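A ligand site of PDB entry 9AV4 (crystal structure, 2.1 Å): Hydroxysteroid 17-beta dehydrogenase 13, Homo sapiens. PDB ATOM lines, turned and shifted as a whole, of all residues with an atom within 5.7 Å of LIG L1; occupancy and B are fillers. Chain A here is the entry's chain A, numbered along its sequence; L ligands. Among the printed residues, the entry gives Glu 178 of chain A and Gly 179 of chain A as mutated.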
ATOM      1  N   ALA A 172      20.934  13.026  -6.713  1.00  0.00           N
ATOM      2  CA  ALA A 172      21.740  11.832  -6.866  1.00  0.00           C
ATOM      3  C   ALA A 172      20.892  10.571  -6.431  1.00  0.00           C
ATOM      4  O   ALA A 172      19.902  10.339  -7.110  1.00  0.00           O
ATOM      5  CB  ALA A 172      23.104  12.011  -6.163  1.00  0.00           C
ATOM      6  N   SER A 173      21.174   9.836  -5.312  1.00  0.00           N
ATOM      7  CA  SER A 173      20.477   8.642  -4.884  1.00  0.00           C
ATOM      8  C   SER A 173      21.272   8.055  -3.707  1.00  0.00           C
ATOM      9  O   SER A 173      22.449   8.428  -3.521  1.00  0.00           O
ATOM     10  CB  SER A 173      20.497   7.632  -6.026  1.00  0.00           C
ATOM     11  OG  SER A 173      20.016   6.358  -5.658  1.00  0.00           O
ATOM     12  N   VAL A 174      20.700   7.070  -2.954  1.00  0.00           N
ATOM     13  CA  VAL A 174      21.521   6.320  -1.979  1.00  0.00           C
ATOM     14  C   VAL A 174      22.605   5.512  -2.750  1.00  0.00           C
ATOM     15  O   VAL A 174      23.664   5.228  -2.180  1.00  0.00           O
ATOM     16  CB  VAL A 174      20.740   5.426  -1.021  1.00  0.00           C
ATOM     17  CG1 VAL A 174      20.073   6.272   0.049  1.00  0.00           C
ATOM     18  CG2 VAL A 174      19.724   4.570  -1.772  1.00  0.00           C
ATOM     19  N   CYS A 175      22.357   5.214  -4.063  1.00  0.00           N
ATOM     20  CA  CYS A 175      23.281   4.589  -5.019  1.00  0.00           C
ATOM     21  C   CYS A 175      24.560   5.425  -5.227  1.00  0.00           C
ATOM     22  O   CYS A 175      25.508   4.901  -5.799  1.00  0.00           O
ATOM     23  CB  CYS A 175      22.591   4.319  -6.350  1.00  0.00           C
ATOM     24  SG  CYS A 175      21.273   3.090  -6.254  1.00  0.00           S
ATOM     25  N   GLU A 178      26.322   3.943  -1.790  1.00  0.00           N
ATOM     26  CA  GLU A 178      26.493   2.510  -1.689  1.00  0.00           C
ATOM     27  C   GLU A 178      26.080   1.821  -3.003  1.00  0.00           C
ATOM     28  O   GLU A 178      25.103   2.222  -3.618  1.00  0.00           O
ATOM     29  CB  GLU A 178      25.693   1.968  -0.489  1.00  0.00           C
ATOM     30  CG  GLU A 178      25.793   0.455  -0.263  1.00  0.00           C
ATOM     31  CD  GLU A 178      27.146  -0.146   0.063  1.00  0.00           C
ATOM     32  OE1 GLU A 178      27.313  -0.634   1.216  1.00  0.00           O
ATOM     33  OE2 GLU A 178      28.032  -0.180  -0.818  1.00  0.00           O
ATOM     34  N   GLY A 179      26.853   0.828  -3.435  1.00  0.00           N
ATOM     35  CA  GLY A 179      26.582   0.097  -4.659  1.00  0.00           C
ATOM     36  C   GLY A 179      25.442  -0.883  -4.542  1.00  0.00           C
ATOM     37  O   GLY A 179      25.037  -1.259  -3.435  1.00  0.00           O
ATOM     38  N   ILE A 180      24.890  -1.292  -5.681  1.00  0.00           N
ATOM     39  CA  ILE A 180      23.779  -2.238  -5.753  1.00  0.00           C
ATOM     40  C   ILE A 180      24.011  -3.195  -6.904  1.00  0.00           C
ATOM     41  O   ILE A 180      24.213  -2.751  -8.029  1.00  0.00           O
ATOM     42  CB  ILE A 180      22.440  -1.466  -5.979  1.00  0.00           C
ATOM     43  CG1 ILE A 180      22.063  -0.587  -4.781  1.00  0.00           C
ATOM     44  CG2 ILE A 180      21.285  -2.412  -6.343  1.00  0.00           C
ATOM     45  CD1 ILE A 180      20.876   0.261  -5.033  1.00  0.00           C
ATOM     46  N   LEU A 183      23.042  -2.735 -10.998  1.00  0.00           N
ATOM     47  CA  LEU A 183      22.950  -1.300 -11.254  1.00  0.00           C
ATOM     48  C   LEU A 183      24.362  -0.691 -11.229  1.00  0.00           C
ATOM     49  O   LEU A 183      24.513   0.425 -10.733  1.00  0.00           O
ATOM     50  CB  LEU A 183      22.025  -0.586 -10.219  1.00  0.00           C
ATOM     51  CG  LEU A 183      20.527  -0.893 -10.293  1.00  0.00           C
ATOM     52  CD1 LEU A 183      19.769  -0.165  -9.189  1.00  0.00           C
ATOM     53  CD2 LEU A 183      19.953  -0.543 -11.645  1.00  0.00           C
ATOM     54  N   TYR A 186      24.804   2.652 -13.268  1.00  0.00           N
ATOM     55  CA  TYR A 186      23.967   3.659 -12.631  1.00  0.00           C
ATOM     56  C   TYR A 186      24.569   4.108 -11.301  1.00  0.00           C
ATOM     57  O   TYR A 186      24.626   5.306 -11.038  1.00  0.00           O
ATOM     58  CB  TYR A 186      22.560   3.104 -12.441  1.00  0.00           C
ATOM     59  CG  TYR A 186      21.644   4.006 -11.655  1.00  0.00           C
ATOM     60  CD1 TYR A 186      20.980   5.050 -12.270  1.00  0.00           C
ATOM     61  CD2 TYR A 186      21.407   3.783 -10.306  1.00  0.00           C
ATOM     62  CE1 TYR A 186      20.106   5.873 -11.567  1.00  0.00           C
ATOM     63  CE2 TYR A 186      20.551   4.606  -9.580  1.00  0.00           C
ATOM     64  CZ  TYR A 186      19.896   5.641 -10.220  1.00  0.00           C
ATOM     65  OH  TYR A 186      19.031   6.443  -9.513  1.00  0.00           O
ATOM     66  N   LYS A 190      25.902   7.785 -10.201  1.00  0.00           N
ATOM     67  CA  LYS A 190      25.352   8.420  -9.001  1.00  0.00           C
ATOM     68  C   LYS A 190      26.452   8.802  -8.020  1.00  0.00           C
ATOM     69  O   LYS A 190      26.364   9.848  -7.374  1.00  0.00           O
ATOM     70  CB  LYS A 190      24.243   7.579  -8.366  1.00  0.00           C
ATOM     71  CG  LYS A 190      22.931   7.611  -9.157  1.00  0.00           C
ATOM     72  CD  LYS A 190      22.399   9.029  -9.307  1.00  0.00           C
ATOM     73  CE  LYS A 190      21.311   9.086 -10.342  1.00  0.00           C
ATOM     74  NZ  LYS A 190      20.466  10.304 -10.214  1.00  0.00           N
ATOM     75  N   PRO A 219      17.611  10.088  -2.207  1.00  0.00           N
ATOM     76  CA  PRO A 219      16.523   9.223  -1.709  1.00  0.00           C
ATOM     77  C   PRO A 219      16.816   7.729  -1.925  1.00  0.00           C
ATOM     78  O   PRO A 219      17.609   7.339  -2.799  1.00  0.00           O
ATOM     79  CB  PRO A 219      15.322   9.635  -2.581  1.00  0.00           C
ATOM     80  CG  PRO A 219      15.841  10.705  -3.552  1.00  0.00           C
ATOM     81  CD  PRO A 219      17.325  10.596  -3.554  1.00  0.00           C
ATOM     82  N   VAL A 220      16.143   6.880  -1.136  1.00  0.00           N
ATOM     83  CA  VAL A 220      16.155   5.438  -1.340  1.00  0.00           C
ATOM     84  C   VAL A 220      15.065   5.176  -2.445  1.00  0.00           C
ATOM     85  O   VAL A 220      14.684   6.128  -3.153  1.00  0.00           O
ATOM     86  CB  VAL A 220      15.915   4.666  -0.010  1.00  0.00           C
ATOM     87  CG1 VAL A 220      16.980   5.003   1.015  1.00  0.00           C
ATOM     88  CG2 VAL A 220      14.529   4.927   0.540  1.00  0.00           C
ATOM     89  N   PHE A 221      14.587   3.947  -2.661  1.00  0.00           N
ATOM     90  CA  PHE A 221      13.585   3.663  -3.673  1.00  0.00           C
ATOM     91  C   PHE A 221      12.312   4.529  -3.536  1.00  0.00           C
ATOM     92  O   PHE A 221      11.636   4.510  -2.501  1.00  0.00           O
ATOM     93  CB  PHE A 221      13.235   2.188  -3.643  1.00  0.00           C
ATOM     94  CG  PHE A 221      12.319   1.784  -4.760  1.00  0.00           C
ATOM     95  CD1 PHE A 221      11.005   1.443  -4.503  1.00  0.00           C
ATOM     96  CD2 PHE A 221      12.749   1.798  -6.070  1.00  0.00           C
ATOM     97  CE1 PHE A 221      10.149   1.087  -5.533  1.00  0.00           C
ATOM     98  CE2 PHE A 221      11.898   1.450  -7.086  1.00  0.00           C
ATOM     99  CZ  PHE A 221      10.604   1.080  -6.818  1.00  0.00           C
ATOM    100  N   PHE A 226      10.613   4.489 -12.125  1.00  0.00           N
ATOM    101  CA  PHE A 226      11.978   4.629 -12.607  1.00  0.00           C
ATOM    102  C   PHE A 226      12.650   3.254 -12.710  1.00  0.00           C
ATOM    103  O   PHE A 226      13.282   2.948 -13.723  1.00  0.00           O
ATOM    104  CB  PHE A 226      12.742   5.592 -11.691  1.00  0.00           C
ATOM    105  CG  PHE A 226      14.103   6.006 -12.186  1.00  0.00           C
ATOM    106  CD1 PHE A 226      14.249   6.770 -13.331  1.00  0.00           C
ATOM    107  CD2 PHE A 226      15.243   5.649 -11.489  1.00  0.00           C
ATOM    108  CE1 PHE A 226      15.498   7.175 -13.761  1.00  0.00           C
ATOM    109  CE2 PHE A 226      16.493   6.036 -11.937  1.00  0.00           C
ATOM    110  CZ  PHE A 226      16.616   6.797 -13.074  1.00  0.00           C
ATOM    111  N   THR A 227      12.493   2.412 -11.661  1.00  0.00           N
ATOM    112  CA  THR A 227      12.834   0.983 -11.623  1.00  0.00           C
ATOM    113  C   THR A 227      11.603   0.240 -11.076  1.00  0.00           C
ATOM    114  O   THR A 227      10.725   0.877 -10.488  1.00  0.00           O
ATOM    115  CB  THR A 227      14.151   0.612 -10.899  1.00  0.00           C
ATOM    116  OG1 THR A 227      14.058   0.881  -9.501  1.00  0.00           O
ATOM    117  CG2 THR A 227      15.368   1.263 -11.505  1.00  0.00           C
ATOM    118  N   ASN A 229      11.209  -2.449  -8.587  1.00  0.00           N
ATOM    119  CA  ASN A 229      11.095  -2.745  -7.151  1.00  0.00           C
ATOM    120  C   ASN A 229      12.367  -2.299  -6.404  1.00  0.00           C
ATOM    121  O   ASN A 229      13.420  -2.159  -7.035  1.00  0.00           O
ATOM    122  CB  ASN A 229      10.934  -4.265  -6.987  1.00  0.00           C
ATOM    123  CG  ASN A 229       9.676  -4.855  -7.575  1.00  0.00           C
ATOM    124  OD1 ASN A 229       8.554  -4.436  -7.258  1.00  0.00           O
ATOM    125  ND2 ASN A 229       9.844  -5.841  -8.440  1.00  0.00           N
ATOM    126  N   PRO A 230      12.319  -2.104  -5.063  1.00  0.00           N
ATOM    127  CA  PRO A 230      13.557  -1.748  -4.342  1.00  0.00           C
ATOM    128  C   PRO A 230      14.543  -2.918  -4.303  1.00  0.00           C
ATOM    129  O   PRO A 230      14.122  -4.079  -4.264  1.00  0.00           O
ATOM    130  CB  PRO A 230      13.063  -1.382  -2.932  1.00  0.00           C
ATOM    131  CG  PRO A 230      11.766  -2.062  -2.794  1.00  0.00           C
ATOM    132  CD  PRO A 230      11.158  -2.222  -4.151  1.00  0.00           C
ATOM    133  N   SER A 231      15.853  -2.635  -4.336  1.00  0.00           N
ATOM    134  CA  SER A 231      16.895  -3.671  -4.359  1.00  0.00           C
ATOM    135  C   SER A 231      17.089  -4.425  -3.017  1.00  0.00           C
ATOM    136  O   SER A 231      17.861  -5.394  -2.957  1.00  0.00           O
ATOM    137  CB  SER A 231      18.212  -3.083  -4.843  1.00  0.00           C
ATOM    138  OG  SER A 231      18.725  -2.186  -3.872  1.00  0.00           O
ATOM    139  N   THR A 232      16.413  -3.975  -1.940  1.00  0.00           N
ATOM    140  CA  THR A 232      16.477  -4.585  -0.593  1.00  0.00           C
ATOM    141  C   THR A 232      15.048  -4.822  -0.034  1.00  0.00           C
ATOM    142  O   THR A 232      14.063  -4.380  -0.645  1.00  0.00           O
ATOM    143  CB  THR A 232      17.318  -3.692   0.365  1.00  0.00           C
ATOM    144  OG1 THR A 232      16.599  -2.494   0.665  1.00  0.00           O
ATOM    145  CG2 THR A 232      18.706  -3.364  -0.183  1.00  0.00           C
ATOM    146  N   ARG A 233      14.925  -5.503   1.144  1.00  0.00           N
ATOM    147  CA  ARG A 233      13.633  -5.735   1.821  1.00  0.00           C
ATOM    148  C   ARG A 233      13.188  -4.470   2.595  1.00  0.00           C
ATOM    149  O   ARG A 233      12.928  -4.511   3.797  1.00  0.00           O
ATOM    150  CB  ARG A 233      13.720  -6.955   2.761  1.00  0.00           C
ATOM    151  CG  ARG A 233      14.168  -8.225   2.040  1.00  0.00           C
ATOM    152  CD  ARG A 233      13.736  -9.509   2.740  1.00  0.00           C
ATOM    153  NE  ARG A 233      14.065 -10.693   1.937  1.00  0.00           N
ATOM    154  CZ  ARG A 233      13.830 -11.943   2.297  1.00  0.00           C
ATOM    155  NH1 ARG A 233      13.278 -12.221   3.476  1.00  0.00           N
ATOM    156  NH2 ARG A 233      14.152 -12.952   1.486  1.00  0.00           N
ATOM    157  N   LEU A 234      13.087  -3.336   1.878  1.00  0.00           N
ATOM    158  CA  LEU A 234      12.724  -2.018   2.387  1.00  0.00           C
ATOM    159  C   LEU A 234      11.239  -1.939   2.742  1.00  0.00           C
ATOM    160  O   LEU A 234      10.377  -1.977   1.867  1.00  0.00           O
ATOM    161  CB  LEU A 234      13.085  -0.971   1.322  1.00  0.00           C
ATOM    162  CG  LEU A 234      12.795   0.487   1.643  1.00  0.00           C
ATOM    163  CD1 LEU A 234      13.497   0.914   2.916  1.00  0.00           C
ATOM    164  CD2 LEU A 234      13.209   1.380   0.490  1.00  0.00           C
ATOM    165  N   TYR A 264      18.670   7.243   6.878  1.00  0.00           N
ATOM    166  CA  TYR A 264      19.588   6.414   6.089  1.00  0.00           C
ATOM    167  C   TYR A 264      21.040   6.842   6.185  1.00  0.00           C
ATOM    168  O   TYR A 264      21.917   6.113   5.722  1.00  0.00           O
ATOM    169  CB  TYR A 264      19.165   6.312   4.636  1.00  0.00           C
ATOM    170  CG  TYR A 264      18.528   4.973   4.400  1.00  0.00           C
ATOM    171  CD1 TYR A 264      19.292   3.850   4.153  1.00  0.00           C
ATOM    172  CD2 TYR A 264      17.160   4.794   4.587  1.00  0.00           C
ATOM    173  CE1 TYR A 264      18.715   2.596   4.028  1.00  0.00           C
ATOM    174  CE2 TYR A 264      16.571   3.555   4.435  1.00  0.00           C
ATOM    175  CZ  TYR A 264      17.347   2.454   4.144  1.00  0.00           C
ATOM    176  OH  TYR A 264      16.768   1.220   3.994  1.00  0.00           O
ATOM    177  N   LEU A 268      24.586   4.206   6.453  1.00  0.00           N
ATOM    178  CA  LEU A 268      25.790   4.464   5.673  1.00  0.00           C
ATOM    179  C   LEU A 268      27.010   4.662   6.579  1.00  0.00           C
ATOM    180  O   LEU A 268      28.111   4.233   6.225  1.00  0.00           O
ATOM    181  CB  LEU A 268      25.581   5.690   4.770  1.00  0.00           C
ATOM    182  CG  LEU A 268      25.034   5.507   3.333  1.00  0.00           C
ATOM    183  CD1 LEU A 268      24.353   4.153   3.076  1.00  0.00           C
ATOM    184  CD2 LEU A 268      24.107   6.606   2.980  1.00  0.00           C
ATOM    185  N   ASP A 271      28.114   1.221   7.841  1.00  0.00           N
ATOM    186  CA  ASP A 271      28.808   0.497   6.766  1.00  0.00           C
ATOM    187  C   ASP A 271      30.305   0.816   6.770  1.00  0.00           C
ATOM    188  O   ASP A 271      31.125  -0.053   6.485  1.00  0.00           O
ATOM    189  CB  ASP A 271      28.212   0.834   5.387  1.00  0.00           C
ATOM    190  CG  ASP A 271      26.964   0.051   5.026  1.00  0.00           C
ATOM    191  OD1 ASP A 271      26.590  -0.863   5.798  1.00  0.00           O
ATOM    192  OD2 ASP A 271      26.378   0.350   3.966  1.00  0.00           O
HETATM  193  C1  LIG L   1      17.057   1.935  -6.904  1.00  0.00           C
HETATM  194  C2  LIG L   1      17.368   2.480  -4.203  1.00  0.00           C
HETATM  195  C3  LIG L   1      17.087   1.188  -4.624  1.00  0.00           C
HETATM  196  C4  LIG L   1      19.415   0.668  -1.917  1.00  0.00           C
HETATM  197  C5  LIG L   1      17.498   4.297  -7.541  1.00  0.00           C
HETATM  198  C6  LIG L   1      19.273   1.613   0.696  1.00  0.00           C
HETATM  199  F1  LIG L   1      17.789   4.693  -4.715  1.00  0.00           F
HETATM  200  C7  LIG L   1      17.497   3.459  -5.147  1.00  0.00           C
HETATM  201  C8  LIG L   1      17.349   3.241  -6.509  1.00  0.00           C
HETATM  202  C9  LIG L   1      16.922   0.923  -5.973  1.00  0.00           C
HETATM  203  N1  LIG L   1      17.026   0.125  -3.675  1.00  0.00           N
HETATM  204  S1  LIG L   1      16.712   0.257  -2.076  1.00  0.00           S
HETATM  205  O1  LIG L   1      16.418  -1.073  -1.643  1.00  0.00           O
HETATM  206  O2  LIG L   1      15.737   1.282  -1.891  1.00  0.00           O
HETATM  207  C10 LIG L   1      18.189   0.785  -1.262  1.00  0.00           C
HETATM  208  C11 LIG L   1      20.562   1.029  -1.243  1.00  0.00           C
HETATM  209  C12 LIG L   1      20.501   1.473   0.075  1.00  0.00           C
HETATM  210  C13 LIG L   1      18.113   1.281   0.021  1.00  0.00           C
HETATM  211 CL1  LIG L   1      21.934   1.791   0.987  1.00  0.00          CL
HETATM  212 CL2  LIG L   1      22.087   0.994  -2.094  1.00  0.00          CL
HETATM  213  O3  LIG L   1      16.834   4.318  -8.563  1.00  0.00           O
HETATM  214  O4  LIG L   1      18.387   5.204  -7.251  1.00  0.00           O
HETATM  215  P1  LG2 L   2      10.930   9.390 -13.590  1.00  0.00           P
HETATM  216  O1  LG2 L   2       9.668   9.627 -12.859  1.00  0.00           O
HETATM  217  O2  LG2 L   2      11.065   8.201 -14.461  1.00  0.00           O
HETATM  218  O3  LG2 L   2      11.216  10.748 -14.378  1.00  0.00           O
HETATM  219  C1  LG2 L   2      12.547  11.178 -14.729  1.00  0.00           C
HETATM  220  C2  LG2 L   2      12.363  12.231 -15.804  1.00  0.00           C
HETATM  221  O4  LG2 L   2      13.628  12.527 -16.436  1.00  0.00           O
HETATM  222  C3  LG2 L   2      11.396  11.785 -16.908  1.00  0.00           C
HETATM  223  O5  LG2 L   2      10.343  12.722 -17.085  1.00  0.00           O
HETATM  224  C4  LG2 L   2      12.306  11.675 -18.139  1.00  0.00           C
HETATM  225  O6  LG2 L   2      11.664  12.059 -19.353  1.00  0.00           O
HETATM  226  C5  LG2 L   2      13.385  12.692 -17.817  1.00  0.00           C
HETATM  227  N1  LG2 L   2      14.614  12.517 -18.569  1.00  0.00           N
HETATM  228  C6  LG2 L   2      15.223  11.330 -18.894  1.00  0.00           C
HETATM  229  N2  LG2 L   2      16.211  11.457 -19.749  1.00  0.00           N
HETATM  230  C7  LG2 L   2      16.260  12.821 -20.002  1.00  0.00           C
HETATM  231  C8  LG2 L   2      17.060  13.596 -20.865  1.00  0.00           C
HETATM  232  N3  LG2 L   2      18.062  13.111 -21.601  1.00  0.00           N
HETATM  233  N4  LG2 L   2      16.819  14.928 -20.912  1.00  0.00           N
HETATM  234  C9  LG2 L   2      15.847  15.430 -20.145  1.00  0.00           C
HETATM  235  N5  LG2 L   2      15.026  14.793 -19.305  1.00  0.00           N
HETATM  236  C10 LG2 L   2      15.286  13.480 -19.282  1.00  0.00           C
HETATM  237  O7  LG2 L   2      12.130   9.393 -12.525  1.00  0.00           O
HETATM  238  P2  LG2 L   2      12.272   9.723 -10.959  1.00  0.00           P
HETATM  239  O8  LG2 L   2      11.572  10.995 -10.640  1.00  0.00           O
HETATM  240  O9  LG2 L   2      12.000   8.512 -10.167  1.00  0.00           O
HETATM  241  O10 LG2 L   2      13.833  10.036 -10.878  1.00  0.00           O
HETATM  242  C11 LG2 L   2      14.321  11.380 -10.971  1.00  0.00           C
HETATM  243  C12 LG2 L   2      15.749  11.416 -10.469  1.00  0.00           C
HETATM  244  O11 LG2 L   2      15.802  10.866  -9.143  1.00  0.00           O
HETATM  245  C13 LG2 L   2      16.759  10.627 -11.302  1.00  0.00           C
HETATM  246  O12 LG2 L   2      17.995  11.328 -11.360  1.00  0.00           O
HETATM  247  C14 LG2 L   2      16.941   9.339 -10.500  1.00  0.00           C
HETATM  248  O13 LG2 L   2      18.209   8.739 -10.727  1.00  0.00           O
HETATM  249  C15 LG2 L   2      16.820   9.893  -9.079  1.00  0.00           C
HETATM  250  N6  LG2 L   2      16.443   8.856  -8.065  1.00  0.00           N
HETATM  251  C16 LG2 L   2      15.406   8.027  -8.291  1.00  0.00           C
HETATM  252  C17 LG2 L   2      15.049   7.084  -7.347  1.00  0.00           C
HETATM  253  C18 LG2 L   2      13.838   6.202  -7.540  1.00  0.00           C
HETATM  254  O14 LG2 L   2      13.749   5.161  -6.896  1.00  0.00           O
HETATM  255  N7  LG2 L   2      12.885   6.625  -8.350  1.00  0.00           N
HETATM  256  C19 LG2 L   2      15.780   7.010  -6.179  1.00  0.00           C
HETATM  257  C20 LG2 L   2      16.837   7.875  -5.960  1.00  0.00           C
HETATM  258  C21 LG2 L   2      17.167   8.789  -6.928  1.00  0.00           C
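An oxygen (O13) of LG2 L2 sits at hydrogen-bond distance from the side-chain hydroxyl (OH) of Tyr 186. A nitrogen (N1) of LIG L1 sits at hydrogen-bond distance from the side-chain hydroxyl (OG) of Ser 231 (2.9 Å). OH of Tyr 186 sits at hydrogen-bond distance from O4 of LIG L1 (2.7 Å). The side-chain sulfur (SG) of Cys 175 is in hydrogen-bond range of an oxygen (O4) of LIG L1 (3.7 Å). O2 of LIG L1 is in hydrogen-bond range of N of Phe 221, 3.0 Å away. The backbone NH (N) of Thr 232 is in hydrogen-bond range of an oxygen (O1) of LIG L1 (2.9 Å). O1 of LIG L1 lies within hydrogen-bond range of N of Ser 231, 3.2 Å away. The side-chain amino group of Lys 190 is in hydrogen-bond range of an oxygen (O13) of LG2 L2. The side-chain hydroxyl (OG1) of Thr 232 sits at hydrogen-bond distance from an oxygen (O1) of LIG L1 (2.7 Å). The side-chain hydroxyl (OG) of Ser 173 is in hydrogen-bond range of an oxygen (O4) of LIG L1 (2.6 Å).
OG of Ser 173 sits at hydrogen-bond distance from N of Cys 175 (3.1 Å). The backbone NH of Val 174 is in hydrogen-bond range of the backbone carbonyl oxygen of Pro 219.
The backbone carbonyl oxygen (O) of Pro 219 sits close to a fluorine (F1) of LIG L1 (3.3 Å). Val 174 touches LIG L1. Glu 178 touches LIG L1. O of Gly 179 touches CL2 of LIG L1, at 3.9 Å. CG1 of Ile 180 touches CL2 of LIG L1, at 3.1 Å. C of Val 220 touches F1 of LIG L1 (3.6 Å). Phe 226 touches LIG L1. Pro 230 touches LIG L1. CD2 of Leu 234 touches O2 of LIG L1 (3.5 Å). CE1 of Tyr 264 touches C6 of LIG L1, 3.5 Å away. Leu 268 touches LIG L1. Of the 24 residues printed, 17 come within 4 Å of LIG L1. Along chain A the residues within 4 Å of LIG L1 span positions 173 to 268. The nearest printed residue that does not touch LIG L1 is Thr 227 (4.1 Å).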
